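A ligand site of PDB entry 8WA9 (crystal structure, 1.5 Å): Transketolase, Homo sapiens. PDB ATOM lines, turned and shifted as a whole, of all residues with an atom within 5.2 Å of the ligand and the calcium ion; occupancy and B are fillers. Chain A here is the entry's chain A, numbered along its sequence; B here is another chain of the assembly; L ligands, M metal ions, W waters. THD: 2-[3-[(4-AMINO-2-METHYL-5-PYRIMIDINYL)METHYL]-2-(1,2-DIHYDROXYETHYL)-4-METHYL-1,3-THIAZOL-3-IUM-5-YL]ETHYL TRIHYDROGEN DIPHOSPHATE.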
ATOM      1  N   HIS A  37      27.218  27.386   5.201  1.00  0.00           N
ATOM      2  CA  HIS A  37      26.328  27.391   4.041  1.00  0.00           C
ATOM      3  C   HIS A  37      25.298  28.514   4.169  1.00  0.00           C
ATOM      4  O   HIS A  37      24.093  28.266   4.221  1.00  0.00           O
ATOM      5  CB  HIS A  37      25.620  26.045   3.916  1.00  0.00           C
ATOM      6  CG  HIS A  37      26.546  24.873   3.793  1.00  0.00           C
ATOM      7  ND1 HIS A  37      27.287  24.407   4.851  1.00  0.00           N
ATOM      8  CD2 HIS A  37      26.823  24.075   2.739  1.00  0.00           C
ATOM      9  CE1 HIS A  37      28.002  23.360   4.451  1.00  0.00           C
ATOM     10  NE2 HIS A  37      27.733  23.142   3.170  1.00  0.00           N
ATOM     11  N   SER A  40      22.330  28.469   1.702  1.00  0.00           N
ATOM     12  CA  SER A  40      21.330  27.442   1.981  1.00  0.00           C
ATOM     13  C   SER A  40      20.445  27.844   3.142  1.00  0.00           C
ATOM     14  O   SER A  40      19.298  27.402   3.237  1.00  0.00           O
ATOM     15  CB  SER A  40      22.007  26.099   2.301  1.00  0.00           C
ATOM     16  OG  SER A  40      22.901  25.702   1.270  1.00  0.00           O
ATOM     17  N   SER A  43      17.671  30.791   1.732  1.00  0.00           N
ATOM     18  CA  SER A  43      16.474  30.410   0.981  1.00  0.00           C
ATOM     19  C   SER A  43      15.353  29.972   1.905  1.00  0.00           C
ATOM     20  O   SER A  43      14.177  30.046   1.513  1.00  0.00           O
ATOM     21  CB  SER A  43      16.791  29.292  -0.020  1.00  0.00           C
ATOM     22  OG  SER A  43      17.341  28.155   0.598  1.00  0.00           O
ATOM     23  N   LYS A  75      17.698  19.050   5.556  1.00  0.00           N
ATOM     24  CA  LYS A  75      18.851  19.682   4.912  1.00  0.00           C
ATOM     25  C   LYS A  75      19.711  20.304   6.018  1.00  0.00           C
ATOM     26  O   LYS A  75      19.726  21.519   6.245  1.00  0.00           O
ATOM     27  CB  LYS A  75      18.409  20.691   3.862  1.00  0.00           C
ATOM     28  CG  LYS A  75      17.260  21.616   4.288  1.00  0.00           C
ATOM     29  CD  LYS A  75      17.045  22.726   3.261  1.00  0.00           C
ATOM     30  CE  LYS A  75      17.968  23.921   3.557  1.00  0.00           C
ATOM     31  NZ  LYS A  75      17.889  24.932   2.440  1.00  0.00           N
ATOM     32  N   HIS A  77      22.769  20.970   6.619  1.00  0.00           N
ATOM     33  CA  HIS A  77      23.781  22.002   6.425  1.00  0.00           C
ATOM     34  C   HIS A  77      23.221  23.408   6.575  1.00  0.00           C
ATOM     35  O   HIS A  77      24.004  24.373   6.591  1.00  0.00           O
ATOM     36  CB  HIS A  77      24.450  21.839   5.060  1.00  0.00           C
ATOM     37  CG  HIS A  77      23.494  21.831   3.915  1.00  0.00           C
ATOM     38  ND1 HIS A  77      22.614  20.803   3.681  1.00  0.00           N
ATOM     39  CD2 HIS A  77      23.282  22.739   2.928  1.00  0.00           C
ATOM     40  CE1 HIS A  77      21.896  21.069   2.592  1.00  0.00           C
ATOM     41  NE2 HIS A  77      22.276  22.243   2.131  1.00  0.00           N
ATOM     42  N   HIS A 110      26.752  20.477  11.557  1.00  0.00           N
ATOM     43  CA  HIS A 110      25.424  19.946  11.282  1.00  0.00           C
ATOM     44  C   HIS A 110      24.769  19.580  12.600  1.00  0.00           C
ATOM     45  O   HIS A 110      25.456  19.397  13.619  1.00  0.00           O
ATOM     46  CB  HIS A 110      25.497  18.713  10.356  1.00  0.00           C
ATOM     47  CG  HIS A 110      26.038  19.024   8.993  1.00  0.00           C
ATOM     48  ND1 HIS A 110      27.392  19.189   8.762  1.00  0.00           N
ATOM     49  CD2 HIS A 110      25.421  19.207   7.803  1.00  0.00           C
ATOM     50  CE1 HIS A 110      27.580  19.459   7.481  1.00  0.00           C
ATOM     51  NE2 HIS A 110      26.405  19.467   6.875  1.00  0.00           N
ATOM     52  N   GLY A 123      22.678  15.647   8.027  1.00  0.00           N
ATOM     53  CA  GLY A 123      23.947  15.967   7.403  1.00  0.00           C
ATOM     54  C   GLY A 123      24.156  15.026   6.246  1.00  0.00           C
ATOM     55  O   GLY A 123      24.719  15.402   5.223  1.00  0.00           O
ATOM     56  N   SER A 124      23.683  13.787   6.399  1.00  0.00           N
ATOM     57  CA  SER A 124      23.557  12.886   5.255  1.00  0.00           C
ATOM     58  C   SER A 124      22.156  13.092   4.692  1.00  0.00           C
ATOM     59  O   SER A 124      21.155  12.753   5.343  1.00  0.00           O
ATOM     60  CB  SER A 124      23.786  11.438   5.635  1.00  0.00           C
ATOM     61  OG  SER A 124      23.486  10.644   4.503  1.00  0.00           O
ATOM     62  N   LEU A 125      22.088  13.654   3.495  1.00  0.00           N
ATOM     63  CA  LEU A 125      20.822  14.150   2.965  1.00  0.00           C
ATOM     64  C   LEU A 125      19.854  13.009   2.702  1.00  0.00           C
ATOM     65  O   LEU A 125      20.237  11.868   2.408  1.00  0.00           O
ATOM     66  CB  LEU A 125      21.059  14.919   1.668  1.00  0.00           C
ATOM     67  CG  LEU A 125      21.761  16.255   1.896  1.00  0.00           C
ATOM     68  CD1 LEU A 125      22.334  16.761   0.594  1.00  0.00           C
ATOM     69  CD2 LEU A 125      20.790  17.248   2.477  1.00  0.00           C
ATOM     70  N   GLY A 154      15.806  20.013   1.219  1.00  0.00           N
ATOM     71  CA  GLY A 154      16.280  20.733   0.056  1.00  0.00           C
ATOM     72  C   GLY A 154      15.762  20.124  -1.235  1.00  0.00           C
ATOM     73  O   GLY A 154      15.150  19.053  -1.217  1.00  0.00           O
ATOM     74  N   ASP A 155      16.012  20.796  -2.364  1.00  0.00           N
ATOM     75  CA  ASP A 155      15.505  20.215  -3.610  1.00  0.00           C
ATOM     76  C   ASP A 155      16.495  19.225  -4.239  1.00  0.00           C
ATOM     77  O   ASP A 155      16.063  18.158  -4.706  1.00  0.00           O
ATOM     78  CB  ASP A 155      15.039  21.292  -4.631  1.00  0.00           C
ATOM     79  CG  ASP A 155      16.067  22.361  -4.963  1.00  0.00           C
ATOM     80  OD1 ASP A 155      17.118  22.436  -4.339  1.00  0.00           O
ATOM     81  OD2 ASP A 155      15.776  23.152  -5.893  1.00  0.00           O
ATOM     82  N   GLY A 156      17.798  19.502  -4.202  1.00  0.00           N
ATOM     83  CA  GLY A 156      18.754  18.472  -4.586  1.00  0.00           C
ATOM     84  C   GLY A 156      18.581  17.217  -3.746  1.00  0.00           C
ATOM     85  O   GLY A 156      18.653  16.095  -4.262  1.00  0.00           O
ATOM     86  N   GLU A 157      18.301  17.404  -2.451  1.00  0.00           N
ATOM     87  CA  GLU A 157      18.059  16.305  -1.524  1.00  0.00           C
ATOM     88  C   GLU A 157      16.965  15.360  -2.003  1.00  0.00           C
ATOM     89  O   GLU A 157      17.018  14.154  -1.704  1.00  0.00           O
ATOM     90  CB  GLU A 157      17.694  16.898  -0.165  1.00  0.00           C
ATOM     91  CG  GLU A 157      17.318  15.865   0.884  1.00  0.00           C
ATOM     92  CD  GLU A 157      17.181  16.448   2.259  1.00  0.00           C
ATOM     93  OE1 GLU A 157      16.881  17.649   2.386  1.00  0.00           O
ATOM     94  OE2 GLU A 157      17.377  15.691   3.224  1.00  0.00           O
ATOM     95  N   GLU A 160      17.367  11.713  -3.434  1.00  0.00           N
ATOM     96  CA  GLU A 160      17.633  10.501  -2.667  1.00  0.00           C
ATOM     97  C   GLU A 160      16.413   9.615  -2.639  1.00  0.00           C
ATOM     98  O   GLU A 160      15.324  10.066  -2.250  1.00  0.00           O
ATOM     99  CB  GLU A 160      18.049  10.825  -1.233  1.00  0.00           C
ATOM    100  CG  GLU A 160      19.448  11.412  -1.107  1.00  0.00           C
ATOM    101  CD  GLU A 160      20.575  10.408  -1.317  1.00  0.00           C
ATOM    102  OE1 GLU A 160      20.338   9.235  -1.647  1.00  0.00           O
ATOM    103  OE2 GLU A 160      21.730  10.824  -1.160  1.00  0.00           O
ATOM    104  N   ASP A 183      12.297  23.138   0.033  1.00  0.00           N
ATOM    105  CA  ASP A 183      12.987  24.394  -0.267  1.00  0.00           C
ATOM    106  C   ASP A 183      13.482  24.305  -1.705  1.00  0.00           C
ATOM    107  O   ASP A 183      14.622  23.929  -1.994  1.00  0.00           O
ATOM    108  CB  ASP A 183      14.120  24.605   0.735  1.00  0.00           C
ATOM    109  CG  ASP A 183      14.842  25.934   0.562  1.00  0.00           C
ATOM    110  OD1 ASP A 183      14.547  26.705  -0.377  1.00  0.00           O
ATOM    111  OD2 ASP A 183      15.727  26.189   1.425  1.00  0.00           O
ATOM    112  N   ASN A 185      14.947  25.883  -4.112  1.00  0.00           N
ATOM    113  CA  ASN A 185      15.757  27.047  -4.430  1.00  0.00           C
ATOM    114  C   ASN A 185      16.573  26.867  -5.716  1.00  0.00           C
ATOM    115  O   ASN A 185      17.506  27.649  -5.958  1.00  0.00           O
ATOM    116  CB  ASN A 185      16.669  27.409  -3.245  1.00  0.00           C
ATOM    117  CG  ASN A 185      17.690  26.344  -2.909  1.00  0.00           C
ATOM    118  OD1 ASN A 185      17.962  25.437  -3.697  1.00  0.00           O
ATOM    119  ND2 ASN A 185      18.263  26.460  -1.723  1.00  0.00           N
ATOM    120  N   ARG A 186      16.233  25.846  -6.515  1.00  0.00           N
ATOM    121  CA  ARG A 186      16.679  25.691  -7.905  1.00  0.00           C
ATOM    122  C   ARG A 186      18.037  25.020  -8.020  1.00  0.00           C
ATOM    123  O   ARG A 186      18.326  24.373  -9.037  1.00  0.00           O
ATOM    124  CB  ARG A 186      16.711  27.036  -8.655  1.00  0.00           C
ATOM    125  CG  ARG A 186      16.749  26.858 -10.168  1.00  0.00           C
ATOM    126  CD  ARG A 186      16.717  28.201 -10.939  1.00  0.00           C
ATOM    127  NE  ARG A 186      17.913  29.008 -10.707  1.00  0.00           N
ATOM    128  CZ  ARG A 186      19.064  28.840 -11.341  1.00  0.00           C
ATOM    129  NH1 ARG A 186      19.230  27.862 -12.236  1.00  0.00           N
ATOM    130  NH2 ARG A 186      20.079  29.657 -11.077  1.00  0.00           N
ATOM    131  N   LEU A 187      18.877  25.151  -7.000  1.00  0.00           N
ATOM    132  CA  LEU A 187      20.290  24.798  -7.097  1.00  0.00           C
ATOM    133  C   LEU A 187      20.646  23.730  -6.077  1.00  0.00           C
ATOM    134  O   LEU A 187      20.143  23.747  -4.947  1.00  0.00           O
ATOM    135  CB  LEU A 187      21.190  26.027  -6.879  1.00  0.00           C
ATOM    136  CG  LEU A 187      20.994  27.184  -7.861  1.00  0.00           C
ATOM    137  CD1 LEU A 187      21.915  28.369  -7.530  1.00  0.00           C
ATOM    138  CD2 LEU A 187      21.234  26.673  -9.281  1.00  0.00           C
ATOM    139  N   GLY A 188      21.503  22.803  -6.469  1.00  0.00           N
ATOM    140  CA  GLY A 188      22.180  21.914  -5.535  1.00  0.00           C
ATOM    141  C   GLY A 188      23.553  22.434  -5.176  1.00  0.00           C
ATOM    142  O   GLY A 188      23.758  23.646  -5.069  1.00  0.00           O
ATOM    143  N   GLN A 189      24.500  21.516  -4.994  1.00  0.00           N
ATOM    144  CA  GLN A 189      25.833  21.933  -4.573  1.00  0.00           C
ATOM    145  C   GLN A 189      26.684  22.392  -5.744  1.00  0.00           C
ATOM    146  O   GLN A 189      27.366  23.416  -5.645  1.00  0.00           O
ATOM    147  CB  GLN A 189      26.553  20.790  -3.843  1.00  0.00           C
ATOM    148  CG  GLN A 189      28.064  21.022  -3.745  1.00  0.00           C
ATOM    149  CD  GLN A 189      28.712  20.134  -2.723  1.00  0.00           C
ATOM    150  OE1 GLN A 189      28.127  19.847  -1.676  1.00  0.00           O
ATOM    151  NE2 GLN A 189      29.935  19.674  -3.007  1.00  0.00           N
ATOM    152  N   LYS A 244      18.146  30.520  -3.860  1.00  0.00           N
ATOM    153  CA  LYS A 244      19.292  30.258  -3.000  1.00  0.00           C
ATOM    154  C   LYS A 244      20.012  31.575  -2.735  1.00  0.00           C
ATOM    155  O   LYS A 244      20.158  32.420  -3.626  1.00  0.00           O
ATOM    156  CB  LYS A 244      20.230  29.249  -3.663  1.00  0.00           C
ATOM    157  CG  LYS A 244      21.111  28.470  -2.663  1.00  0.00           C
ATOM    158  CD  LYS A 244      21.658  27.184  -3.287  1.00  0.00           C
ATOM    159  CE  LYS A 244      22.482  26.400  -2.281  1.00  0.00           C
ATOM    160  NZ  LYS A 244      22.657  24.994  -2.755  1.00  0.00           N
ATOM    161  N   HIS A 258      27.478  27.454  -3.126  1.00  0.00           N
ATOM    162  CA  HIS A 258      27.081  26.464  -2.132  1.00  0.00           C
ATOM    163  C   HIS A 258      28.226  26.191  -1.156  1.00  0.00           C
ATOM    164  O   HIS A 258      29.344  25.861  -1.559  1.00  0.00           O
ATOM    165  CB  HIS A 258      26.659  25.148  -2.786  1.00  0.00           C
ATOM    166  CG  HIS A 258      26.248  24.109  -1.787  1.00  0.00           C
ATOM    167  ND1 HIS A 258      24.965  23.998  -1.303  1.00  0.00           N
ATOM    168  CD2 HIS A 258      26.974  23.164  -1.137  1.00  0.00           C
ATOM    169  CE1 HIS A 258      24.901  23.013  -0.427  1.00  0.00           C
ATOM    170  NE2 HIS A 258      26.113  22.500  -0.289  1.00  0.00           N
ATOM    171  N   ASP A 398      23.994   3.785   5.801  1.00  0.00           N
ATOM    172  CA  ASP A 398      24.111   5.217   6.096  1.00  0.00           C
ATOM    173  C   ASP A 398      23.082   5.646   7.143  1.00  0.00           C
ATOM    174  O   ASP A 398      23.369   6.504   8.000  1.00  0.00           O
ATOM    175  CB  ASP A 398      23.936   5.997   4.791  1.00  0.00           C
ATOM    176  CG  ASP A 398      24.375   7.463   4.887  1.00  0.00           C
ATOM    177  OD1 ASP A 398      25.113   7.845   5.817  1.00  0.00           O
ATOM    178  OD2 ASP A 398      23.984   8.236   3.979  1.00  0.00           O
ATOM    179  N   GLY B 340      28.150  12.323  -7.528  1.00  0.00           N
ATOM    180  CA  GLY B 340      26.832  12.628  -6.991  1.00  0.00           C
ATOM    181  C   GLY B 340      26.664  14.031  -6.431  1.00  0.00           C
ATOM    182  O   GLY B 340      26.502  14.215  -5.225  1.00  0.00           O
ATOM    183  N   ASP B 341      26.692  15.022  -7.327  1.00  0.00           N
ATOM    184  CA  ASP B 341      26.587  16.451  -7.007  1.00  0.00           C
ATOM    185  C   ASP B 341      27.685  16.891  -6.056  1.00  0.00           C
ATOM    186  O   ASP B 341      27.522  17.845  -5.304  1.00  0.00           O
ATOM    187  CB  ASP B 341      25.208  16.819  -6.447  1.00  0.00           C
ATOM    188  CG  ASP B 341      24.967  18.326  -6.377  1.00  0.00           C
ATOM    189  OD1 ASP B 341      25.528  19.069  -7.215  1.00  0.00           O
ATOM    190  OD2 ASP B 341      24.200  18.762  -5.497  1.00  0.00           O
ATOM    191  N   THR B 342      28.830  16.200  -6.070  1.00  0.00           N
ATOM    192  CA  THR B 342      29.950  16.619  -5.230  1.00  0.00           C
ATOM    193  C   THR B 342      31.210  16.877  -6.050  1.00  0.00           C
ATOM    194  O   THR B 342      32.302  16.888  -5.480  1.00  0.00           O
ATOM    195  CB  THR B 342      30.229  15.588  -4.121  1.00  0.00           C
ATOM    196  OG1 THR B 342      30.353  14.274  -4.666  1.00  0.00           O
ATOM    197  CG2 THR B 342      29.105  15.585  -3.097  1.00  0.00           C
ATOM    198  N   ILE B 364      22.174  13.612  -6.218  1.00  0.00           N
ATOM    199  CA  ILE B 364      22.371  13.187  -4.816  1.00  0.00           C
ATOM    200  C   ILE B 364      21.618  11.863  -4.671  1.00  0.00           C
ATOM    201  O   ILE B 364      20.490  11.775  -4.170  1.00  0.00           O
ATOM    202  CB  ILE B 364      21.913  14.251  -3.816  1.00  0.00           C
ATOM    203  CG1 ILE B 364      22.586  15.604  -4.136  1.00  0.00           C
ATOM    204  CG2 ILE B 364      22.267  13.850  -2.420  1.00  0.00           C
ATOM    205  CD1 ILE B 364      22.127  16.769  -3.219  1.00  0.00           C
ATOM    206  N   GLU B 366      23.462   8.172  -4.327  1.00  0.00           N
ATOM    207  CA  GLU B 366      24.642   7.320  -4.340  1.00  0.00           C
ATOM    208  C   GLU B 366      24.315   5.879  -4.695  1.00  0.00           C
ATOM    209  O   GLU B 366      25.113   5.205  -5.363  1.00  0.00           O
ATOM    210  CB  GLU B 366      25.344   7.373  -2.980  1.00  0.00           C
ATOM    211  CG  GLU B 366      25.855   8.757  -2.597  1.00  0.00           C
ATOM    212  CD  GLU B 366      24.772   9.704  -2.097  1.00  0.00           C
ATOM    213  OE1 GLU B 366      23.658   9.233  -1.713  1.00  0.00           O
ATOM    214  OE2 GLU B 366      25.051  10.925  -2.057  1.00  0.00           O
ATOM    215  N   THR B 388      32.235  10.410  -4.536  1.00  0.00           N
ATOM    216  CA  THR B 388      31.451  11.199  -3.579  1.00  0.00           C
ATOM    217  C   THR B 388      32.301  11.258  -2.306  1.00  0.00           C
ATOM    218  O   THR B 388      33.461  10.816  -2.315  1.00  0.00           O
ATOM    219  CB  THR B 388      30.050  10.612  -3.337  1.00  0.00           C
ATOM    220  OG1 THR B 388      29.346  11.428  -2.403  1.00  0.00           O
ATOM    221  CG2 THR B 388      30.119   9.185  -2.768  1.00  0.00           C
ATOM    222  N   PHE B 389      31.757  11.829  -1.229  1.00  0.00           N
ATOM    223  CA  PHE B 389      32.419  11.678   0.057  1.00  0.00           C
ATOM    224  C   PHE B 389      32.402  10.206   0.443  1.00  0.00           C
ATOM    225  O   PHE B 389      31.378   9.526   0.280  1.00  0.00           O
ATOM    226  CB  PHE B 389      31.693  12.460   1.160  1.00  0.00           C
ATOM    227  CG  PHE B 389      31.770  13.958   1.063  1.00  0.00           C
ATOM    228  CD1 PHE B 389      31.882  14.621  -0.158  1.00  0.00           C
ATOM    229  CD2 PHE B 389      31.683  14.718   2.213  1.00  0.00           C
ATOM    230  CE1 PHE B 389      31.925  16.013  -0.201  1.00  0.00           C
ATOM    231  CE2 PHE B 389      31.714  16.104   2.164  1.00  0.00           C
ATOM    232  CZ  PHE B 389      31.837  16.751   0.953  1.00  0.00           C
ATOM    233  N   PHE B 392      29.392   8.904   2.266  1.00  0.00           N
ATOM    234  CA  PHE B 392      28.136   8.640   1.559  1.00  0.00           C
ATOM    235  C   PHE B 392      28.201   7.389   0.691  1.00  0.00           C
ATOM    236  O   PHE B 392      27.155   6.966   0.155  1.00  0.00           O
ATOM    237  CB  PHE B 392      27.729   9.887   0.757  1.00  0.00           C
ATOM    238  CG  PHE B 392      27.668  11.114   1.621  1.00  0.00           C
ATOM    239  CD1 PHE B 392      27.130  11.036   2.895  1.00  0.00           C
ATOM    240  CD2 PHE B 392      28.195  12.338   1.189  1.00  0.00           C
ATOM    241  CE1 PHE B 392      27.099  12.148   3.722  1.00  0.00           C
ATOM    242  CE2 PHE B 392      28.155  13.455   2.034  1.00  0.00           C
ATOM    243  CZ  PHE B 392      27.609  13.348   3.299  1.00  0.00           C
ATOM    244  N   ARG B 395      25.838   4.830   1.958  1.00  0.00           N
ATOM    245  CA  ARG B 395      24.491   4.842   1.425  1.00  0.00           C
ATOM    246  C   ARG B 395      24.306   3.769   0.362  1.00  0.00           C
ATOM    247  O   ARG B 395      23.173   3.310   0.157  1.00  0.00           O
ATOM    248  CB  ARG B 395      24.181   6.219   0.836  1.00  0.00           C
ATOM    249  CG  ARG B 395      22.722   6.508   0.511  1.00  0.00           C
ATOM    250  CD  ARG B 395      21.817   6.365   1.727  1.00  0.00           C
ATOM    251  NE  ARG B 395      20.653   7.243   1.615  1.00  0.00           N
ATOM    252  CZ  ARG B 395      20.663   8.515   1.976  1.00  0.00           C
ATOM    253  NH1 ARG B 395      21.743   9.077   2.485  1.00  0.00           N
ATOM    254  NH2 ARG B 395      19.563   9.252   1.794  1.00  0.00           N
ATOM    255  N   ASP B 424      32.904  20.441   9.340  1.00  0.00           N
ATOM    256  CA  ASP B 424      31.593  19.902   8.972  1.00  0.00           C
ATOM    257  C   ASP B 424      31.054  18.947  10.034  1.00  0.00           C
ATOM    258  O   ASP B 424      29.836  18.838  10.194  1.00  0.00           O
ATOM    259  CB  ASP B 424      31.664  19.206   7.614  1.00  0.00           C
ATOM    260  CG  ASP B 424      31.272  20.103   6.457  1.00  0.00           C
ATOM    261  OD1 ASP B 424      30.878  21.272   6.669  1.00  0.00           O
ATOM    262  OD2 ASP B 424      31.364  19.619   5.311  1.00  0.00           O
ATOM    263  N   GLN B 428      29.706  14.086   7.818  1.00  0.00           N
ATOM    264  CA  GLN B 428      30.500  14.083   6.604  1.00  0.00           C
ATOM    265  C   GLN B 428      31.785  13.291   6.733  1.00  0.00           C
ATOM    266  O   GLN B 428      32.527  13.201   5.756  1.00  0.00           O
ATOM    267  CB  GLN B 428      30.849  15.517   6.190  1.00  0.00           C
ATOM    268  CG  GLN B 428      29.725  16.518   6.392  1.00  0.00           C
ATOM    269  CD  GLN B 428      28.590  16.319   5.421  1.00  0.00           C
ATOM    270  OE1 GLN B 428      28.786  16.296   4.204  1.00  0.00           O
ATOM    271  NE2 GLN B 428      27.385  16.169   5.955  1.00  0.00           N
HETATM  272  N1' THD L   1      25.172  13.016  -0.310  1.00  0.00           N
HETATM  273  C2' THD L   1      24.580  13.009   0.883  1.00  0.00           C
HETATM  274  CM2 THD L   1      23.765  11.691   1.191  1.00  0.00           C
HETATM  275  N3' THD L   1      24.560  13.938   1.773  1.00  0.00           N
HETATM  276  C4' THD L   1      25.325  15.013   1.396  1.00  0.00           C
HETATM  277  N4' THD L   1      25.315  15.880   2.467  1.00  0.00           N
HETATM  278  C5' THD L   1      25.944  15.073   0.203  1.00  0.00           C
HETATM  279  C6' THD L   1      25.908  14.116  -0.662  1.00  0.00           C
HETATM  280  C7' THD L   1      26.863  16.240  -0.164  1.00  0.00           C
HETATM  281  N3  THD L   1      26.181  17.595  -0.144  1.00  0.00           N
HETATM  282  C2  THD L   1      25.994  18.348   1.037  1.00  0.00           C
HETATM  283  S1  THD L   1      24.761  19.605   0.820  1.00  0.00           S
HETATM  284  C5  THD L   1      24.519  19.175  -0.890  1.00  0.00           C
HETATM  285  C4  THD L   1      25.373  18.038  -1.174  1.00  0.00           C
HETATM  286  CM4 THD L   1      25.479  17.503  -2.484  1.00  0.00           C
HETATM  287  C6  THD L   1      23.682  19.865  -1.845  1.00  0.00           C
HETATM  288  C7  THD L   1      22.320  20.034  -1.102  1.00  0.00           C
HETATM  289  O7  THD L   1      21.550  20.670  -2.125  1.00  0.00           O
HETATM  290  PA  THD L   1      20.022  20.900  -1.758  1.00  0.00           P
HETATM  291  O1A THD L   1      19.302  19.724  -1.206  1.00  0.00           O
HETATM  292  O2A THD L   1      19.370  21.467  -2.899  1.00  0.00           O
HETATM  293  O3A THD L   1      19.959  21.926  -0.523  1.00  0.00           O
HETATM  294  PB  THD L   1      20.205  23.585  -0.539  1.00  0.00           P
HETATM  295  O1B THD L   1      19.104  24.117   0.296  1.00  0.00           O
HETATM  296  O2B THD L   1      21.572  23.807   0.063  1.00  0.00           O
HETATM  297  O3B THD L   1      20.165  24.079  -1.934  1.00  0.00           O
HETATM  298  C8  THD L   1      26.950  18.567   2.164  1.00  0.00           C
HETATM  299  O9  THD L   1      28.164  17.653   2.252  1.00  0.00           O
HETATM  300  C9  THD L   1      26.745  19.384   3.342  1.00  0.00           C
HETATM  301  O10 THD L   1      25.975  18.498   4.338  1.00  0.00           O
HETATM  302 CA    CA M   1      18.699  23.453  -3.420  1.00  0.00          CA
HETATM  303  O   HOH W   1      17.283  23.411  -1.662  1.00  0.00           O
HETATM  304  O   HOH W   2      23.222  18.123   4.593  1.00  0.00           O
HETATM  305  O   HOH W   3      27.099  12.381  -3.296  1.00  0.00           O
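O2B of the ligand sits at hydrogen-bond distance from NE2 of His 77 (2.7 Å). N of Gly 156 lies within hydrogen-bond range of O1A of the ligand (3.4 Å). The backbone carbonyl oxygen (O) of Gly 123 sits at hydrogen-bond distance from a nitrogen (N4') of the ligand, 2.9 Å away. OE2 of Glu 366 of chain B lies within hydrogen-bond range of N1' of the ligand (2.7 Å). NZ of Lys 75 is in salt-bridge range of O1B of the ligand, 2.6 Å away. NZ of Lys 244 is in salt-bridge range of O2B of the ligand. The side-chain amide oxygen (OE1) of Gln 189 sits close to a nitrogen (N3) of the ligand (3.3 Å). The backbone NH (N) of Glu 157 lies within hydrogen-bond range of an oxygen (O1A) of the ligand (2.8 Å). The side-chain hydroxyl (OG) of Ser 40 lies within hydrogen-bond range of an oxygen (O2B) of the ligand, 2.6 Å away. The backbone NH of Asp 155 sits close to an oxygen (O2A) of the ligand, 3.5 Å away. OE1 of Gln 428 of chain B lies within hydrogen-bond range of O9 of the ligand (2.5 Å). A ring nitrogen (NE2) of His 258 sits close to a sulfur (S1) of the ligand (3.4 Å). A nitrogen (N3') of the ligand lies within hydrogen-bond range of the backbone NH (N) of Leu 125. A ring nitrogen (NE2) of His 110 sits at hydrogen-bond distance from an oxygen (O10) of the ligand (2.7 Å).
The side-chain carboxylate (OE1) of Glu 160 is in salt-bridge range of the guanidinium group (NH2) of Arg 395 of chain B, 3.5 Å away. The backbone carbonyl oxygen of Asp 183 is in hydrogen-bond range of the backbone NH of Asp 155, at 3.4 Å. The backbone carbonyl oxygen (O) of Asp 424 of chain B sits at hydrogen-bond distance from a ring nitrogen (ND1) of His 110, 2.9 Å away. The side-chain hydroxyl of Ser 124 is in hydrogen-bond range of the side-chain carboxylate of Asp 398, at 2.5 Å. The side-chain carboxylate (OE1) of Glu 366 of chain B lies close to the side-chain carboxylate (OE2) of Glu 160 (2.6 Å). The side-chain amide nitrogen (ND2) of Asn 185 is in hydrogen-bond range of the side-chain hydroxyl (OG) of Ser 43, at 3.0 Å. The guanidinium group of Arg 395 of chain B is in salt-bridge range of the side-chain carboxylate of Asp 398 (2.8 Å). The backbone carbonyl oxygen (O) of Leu 125 sits at hydrogen-bond distance from the guanidinium group (NH2) of Arg 395 of chain B (2.8 Å).
Merely in contact with the ligand: His 37, Ser 124, Gly 154, Glu 160, Gly 188, Asp 341 of chain B, Thr 342 of chain B, Ile 364 of chain B, Phe 389 of chain B, Phe 392 of chain B and Arg 395 of chain B. The nearest printed residue that does not touch the ligand is Asp 183 (4.1 Å).
Of the 34 residues printed, 3 come within 4 Å of the calcium ion.
The side-chain carboxylate (OD1) of Asp 155 is bound to the calcium ion (2.1 Å). The backbone carbonyl oxygen (O) of Leu 187 is bound to the calcium ion (2.1 Å). OD1 of Asn 185 is bound to the calcium ion, 2.1 Å away. An oxygen (O2A) of the ligand is bound to the calcium ion (2.2 Å). O3B of the ligand binds the calcium ion (2.2 Å). Water W1 binds the calcium ion. The calcium ion has six donor atoms within binding distance.
Water W1 lies within hydrogen-bond range of the backbone carbonyl oxygen of Asp 183 (2.7 Å), an oxygen (O1B) of the ligand (2.8 Å), the backbone NH of Asp 155 (3.0 Å) and the side-chain amide nitrogen of Asn 185 (3.2 Å). Water W2 lies within hydrogen-bond range of O10 of the ligand, ND1 of His 77 and O of Gly 123. Water W3 lies within hydrogen-bond range of OG1 of Thr 388 of chain B, O of Gly 340 of chain B and OE2 of Glu 366 of chain B.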
